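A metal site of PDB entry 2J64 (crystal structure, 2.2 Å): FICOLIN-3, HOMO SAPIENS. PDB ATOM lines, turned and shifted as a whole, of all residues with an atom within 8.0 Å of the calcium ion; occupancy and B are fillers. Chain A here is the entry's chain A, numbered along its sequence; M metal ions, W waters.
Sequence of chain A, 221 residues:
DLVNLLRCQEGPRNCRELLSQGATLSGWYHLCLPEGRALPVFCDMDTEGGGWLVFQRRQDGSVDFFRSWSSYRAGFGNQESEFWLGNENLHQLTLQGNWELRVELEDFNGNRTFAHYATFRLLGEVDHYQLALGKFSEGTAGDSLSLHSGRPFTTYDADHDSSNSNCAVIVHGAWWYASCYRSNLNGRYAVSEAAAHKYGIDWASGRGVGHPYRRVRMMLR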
ATOM      1  N   THR A 154      21.003 -10.219 -14.825  1.00  0.00           N
ATOM      2  CA  THR A 154      21.805  -8.977 -14.843  1.00  0.00           C
ATOM      3  C   THR A 154      21.262  -7.893 -13.938  1.00  0.00           C
ATOM      4  O   THR A 154      20.043  -7.708 -13.833  1.00  0.00           O
ATOM      5  CB  THR A 154      22.083  -8.378 -16.273  1.00  0.00           C
ATOM      6  OG1 THR A 154      21.317  -7.186 -16.491  1.00  0.00           O
ATOM      7  CG2 THR A 154      21.846  -9.356 -17.343  1.00  0.00           C
ATOM      8  N   ALA A 158      26.046  -5.308 -12.890  1.00  0.00           N
ATOM      9  CA  ALA A 158      26.498  -6.583 -13.463  1.00  0.00           C
ATOM     10  C   ALA A 158      25.755  -6.860 -14.743  1.00  0.00           C
ATOM     11  O   ALA A 158      24.771  -7.584 -14.743  1.00  0.00           O
ATOM     12  CB  ALA A 158      26.295  -7.714 -12.488  1.00  0.00           C
ATOM     13  N   ASP A 159      26.241  -6.278 -15.844  1.00  0.00           N
ATOM     14  CA  ASP A 159      25.539  -6.358 -17.118  1.00  0.00           C
ATOM     15  C   ASP A 159      25.960  -7.604 -17.898  1.00  0.00           C
ATOM     16  O   ASP A 159      27.120  -7.744 -18.285  1.00  0.00           O
ATOM     17  CB  ASP A 159      25.799  -5.079 -17.924  1.00  0.00           C
ATOM     18  CG  ASP A 159      25.171  -5.114 -19.319  1.00  0.00           C
ATOM     19  OD1 ASP A 159      24.547  -6.134 -19.696  1.00  0.00           O
ATOM     20  OD2 ASP A 159      25.322  -4.091 -20.035  1.00  0.00           O
ATOM     21  N   HIS A 160      25.033  -8.543 -18.098  1.00  0.00           N
ATOM     22  CA  HIS A 160      25.363  -9.791 -18.765  1.00  0.00           C
ATOM     23  C   HIS A 160      24.389 -10.077 -19.861  1.00  0.00           C
ATOM     24  O   HIS A 160      24.342 -11.190 -20.384  1.00  0.00           O
ATOM     25  CB  HIS A 160      25.308 -10.975 -17.792  1.00  0.00           C
ATOM     26  CG  HIS A 160      26.096 -10.780 -16.541  1.00  0.00           C
ATOM     27  ND1 HIS A 160      27.470 -10.760 -16.516  1.00  0.00           N
ATOM     28  CD2 HIS A 160      25.682 -10.606 -15.268  1.00  0.00           C
ATOM     29  CE1 HIS A 160      27.879 -10.588 -15.273  1.00  0.00           C
ATOM     30  NE2 HIS A 160      26.817 -10.487 -14.497  1.00  0.00           N
ATOM     31  N   ASP A 161      23.580  -9.092 -20.212  1.00  0.00           N
ATOM     32  CA  ASP A 161      22.512  -9.362 -21.148  1.00  0.00           C
ATOM     33  C   ASP A 161      23.038  -9.363 -22.594  1.00  0.00           C
ATOM     34  O   ASP A 161      24.239  -9.443 -22.838  1.00  0.00           O
ATOM     35  CB  ASP A 161      21.402  -8.345 -20.956  1.00  0.00           C
ATOM     36  CG  ASP A 161      21.891  -6.918 -21.052  1.00  0.00           C
ATOM     37  OD1 ASP A 161      22.531  -6.572 -22.074  1.00  0.00           O
ATOM     38  OD2 ASP A 161      21.625  -6.146 -20.112  1.00  0.00           O
ATOM     39  N   SER A 162      22.121  -9.277 -23.552  1.00  0.00           N
ATOM     40  CA  SER A 162      22.510  -9.415 -24.937  1.00  0.00           C
ATOM     41  C   SER A 162      22.241  -8.082 -25.638  1.00  0.00           C
ATOM     42  O   SER A 162      22.197  -8.000 -26.857  1.00  0.00           O
ATOM     43  CB  SER A 162      21.735 -10.571 -25.598  1.00  0.00           C
ATOM     44  OG  SER A 162      20.338 -10.393 -25.466  1.00  0.00           O
ATOM     45  N   SER A 163      22.065  -7.046 -24.823  1.00  0.00           N
ATOM     46  CA  SER A 163      21.854  -5.717 -25.327  1.00  0.00           C
ATOM     47  C   SER A 163      23.197  -5.010 -25.334  1.00  0.00           C
ATOM     48  O   SER A 163      24.103  -5.390 -24.610  1.00  0.00           O
ATOM     49  CB  SER A 163      20.866  -4.971 -24.427  1.00  0.00           C
ATOM     50  OG  SER A 163      20.755  -3.621 -24.822  1.00  0.00           O
ATOM     51  N   ASN A 164      23.336  -3.998 -26.176  1.00  0.00           N
ATOM     52  CA  ASN A 164      24.590  -3.243 -26.195  1.00  0.00           C
ATOM     53  C   ASN A 164      24.499  -2.132 -25.160  1.00  0.00           C
ATOM     54  O   ASN A 164      25.404  -1.310 -25.036  1.00  0.00           O
ATOM     55  CB  ASN A 164      24.911  -2.700 -27.595  1.00  0.00           C
ATOM     56  CG  ASN A 164      23.973  -1.602 -28.018  1.00  0.00           C
ATOM     57  OD1 ASN A 164      22.782  -1.833 -28.226  1.00  0.00           O
ATOM     58  ND2 ASN A 164      24.510  -0.398 -28.156  1.00  0.00           N
ATOM     59  N   SER A 165      23.385  -2.124 -24.437  1.00  0.00           N
ATOM     60  CA  SER A 165      23.269  -1.326 -23.229  1.00  0.00           C
ATOM     61  C   SER A 165      22.939  -2.250 -22.042  1.00  0.00           C
ATOM     62  O   SER A 165      22.854  -3.489 -22.187  1.00  0.00           O
ATOM     63  CB  SER A 165      22.209  -0.249 -23.390  1.00  0.00           C
ATOM     64  OG  SER A 165      20.911  -0.791 -23.207  1.00  0.00           O
ATOM     65  N   ASN A 166      22.757  -1.654 -20.867  1.00  0.00           N
ATOM     66  CA  ASN A 166      22.434  -2.390 -19.648  1.00  0.00           C
ATOM     67  C   ASN A 166      20.938  -2.323 -19.343  1.00  0.00           C
ATOM     68  O   ASN A 166      20.433  -1.306 -18.871  1.00  0.00           O
ATOM     69  CB  ASN A 166      23.261  -1.854 -18.472  1.00  0.00           C
ATOM     70  CG  ASN A 166      22.862  -2.456 -17.143  1.00  0.00           C
ATOM     71  OD1 ASN A 166      21.704  -2.848 -16.944  1.00  0.00           O
ATOM     72  ND2 ASN A 166      23.811  -2.531 -16.220  1.00  0.00           N
ATOM     73  N   CYS A 167      20.243  -3.437 -19.612  1.00  0.00           N
ATOM     74  CA  CYS A 167      18.774  -3.533 -19.477  1.00  0.00           C
ATOM     75  C   CYS A 167      18.256  -3.277 -18.058  1.00  0.00           C
ATOM     76  O   CYS A 167      17.146  -2.761 -17.888  1.00  0.00           O
ATOM     77  CB  CYS A 167      18.295  -4.915 -19.897  1.00  0.00           C
ATOM     78  SG  CYS A 167      18.282  -5.211 -21.663  1.00  0.00           S
ATOM     79  N   ALA A 168      19.032  -3.691 -17.062  1.00  0.00           N
ATOM     80  CA  ALA A 168      18.669  -3.436 -15.686  1.00  0.00           C
ATOM     81  C   ALA A 168      18.463  -1.941 -15.523  1.00  0.00           C
ATOM     82  O   ALA A 168      17.449  -1.497 -14.993  1.00  0.00           O
ATOM     83  CB  ALA A 168      19.742  -3.951 -14.747  1.00  0.00           C
ATOM     84  N   TYR A 177      17.577 -10.699 -18.190  1.00  0.00           N
ATOM     85  CA  TYR A 177      17.344  -9.900 -19.391  1.00  0.00           C
ATOM     86  C   TYR A 177      17.973 -10.461 -20.674  1.00  0.00           C
ATOM     87  O   TYR A 177      19.070 -11.004 -20.659  1.00  0.00           O
ATOM     88  CB  TYR A 177      17.807  -8.447 -19.181  1.00  0.00           C
ATOM     89  CG  TYR A 177      16.988  -7.741 -18.117  1.00  0.00           C
ATOM     90  CD1 TYR A 177      15.625  -7.615 -18.267  1.00  0.00           C
ATOM     91  CD2 TYR A 177      17.576  -7.214 -16.966  1.00  0.00           C
ATOM     92  CE1 TYR A 177      14.863  -6.988 -17.328  1.00  0.00           C
ATOM     93  CE2 TYR A 177      16.804  -6.561 -16.008  1.00  0.00           C
ATOM     94  CZ  TYR A 177      15.437  -6.458 -16.194  1.00  0.00           C
ATOM     95  OH  TYR A 177      14.611  -5.850 -15.277  1.00  0.00           O
ATOM     96  N   ALA A 178      17.230 -10.312 -21.760  1.00  0.00           N
ATOM     97  CA  ALA A 178      17.780 -10.449 -23.106  1.00  0.00           C
ATOM     98  C   ALA A 178      18.036  -9.025 -23.625  1.00  0.00           C
ATOM     99  O   ALA A 178      19.082  -8.424 -23.320  1.00  0.00           O
ATOM    100  CB  ALA A 178      16.792 -11.179 -23.999  1.00  0.00           C
ATOM    101  N   SER A 179      17.079  -8.460 -24.358  1.00  0.00           N
ATOM    102  CA  SER A 179      17.149  -7.027 -24.667  1.00  0.00           C
ATOM    103  C   SER A 179      15.807  -6.450 -25.094  1.00  0.00           C
ATOM    104  O   SER A 179      15.628  -6.053 -26.243  1.00  0.00           O
ATOM    105  CB  SER A 179      18.218  -6.730 -25.718  1.00  0.00           C
ATOM    106  OG  SER A 179      17.928  -7.377 -26.930  1.00  0.00           O
ATOM    107  N   CYS A 180      14.891  -6.335 -24.127  1.00  0.00           N
ATOM    108  CA  CYS A 180      15.246  -6.615 -22.736  1.00  0.00           C
ATOM    109  C   CYS A 180      14.437  -7.735 -22.091  1.00  0.00           C
ATOM    110  O   CYS A 180      15.020  -8.643 -21.484  1.00  0.00           O
ATOM    111  CB  CYS A 180      15.219  -5.326 -21.905  1.00  0.00           C
ATOM    112  SG  CYS A 180      16.606  -4.209 -22.308  1.00  0.00           S
HETATM  113 CA    CA M   1      24.390  -5.342 -22.184  1.00  0.00          CA
HETATM  114  O   HOH W   1      26.555  -4.203 -22.686  1.00  0.00           O
HETATM  115  O   HOH W   2      25.651  -7.013 -22.614  1.00  0.00           O
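The calcium ion is bound by water W2 (2.1 Å), OD1 of Asp 161 (2.2 Å), O of Ser 165 (2.4 Å), O of Ser 163 (2.4 Å), water W1 (2.5 Å), OD1 of Asp 159 (2.6 Å) and OD2 of Asp 159 (2.7 Å). The calcium ion has seven donor atoms within binding distance.
The side-chain carboxylate of Asp 161 sits at hydrogen-bond distance from the backbone NH of Cys 167 (3.1 Å). The side-chain sulfur (SG) of Cys 167 forms a disulfide with the side-chain sulfur (SG) of Cys 180, at 2.1 Å. The backbone NH (N) of Ser 165 sits close to the side-chain hydroxyl (OG) of Ser 163, 3.1 Å away.
Within 4 Å of the calcium ion: Asp 159, Asp 161, Ser 163 and Ser 165. The nearest printed residue that does not touch the calcium ion is Asn 166 (4.2 Å).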
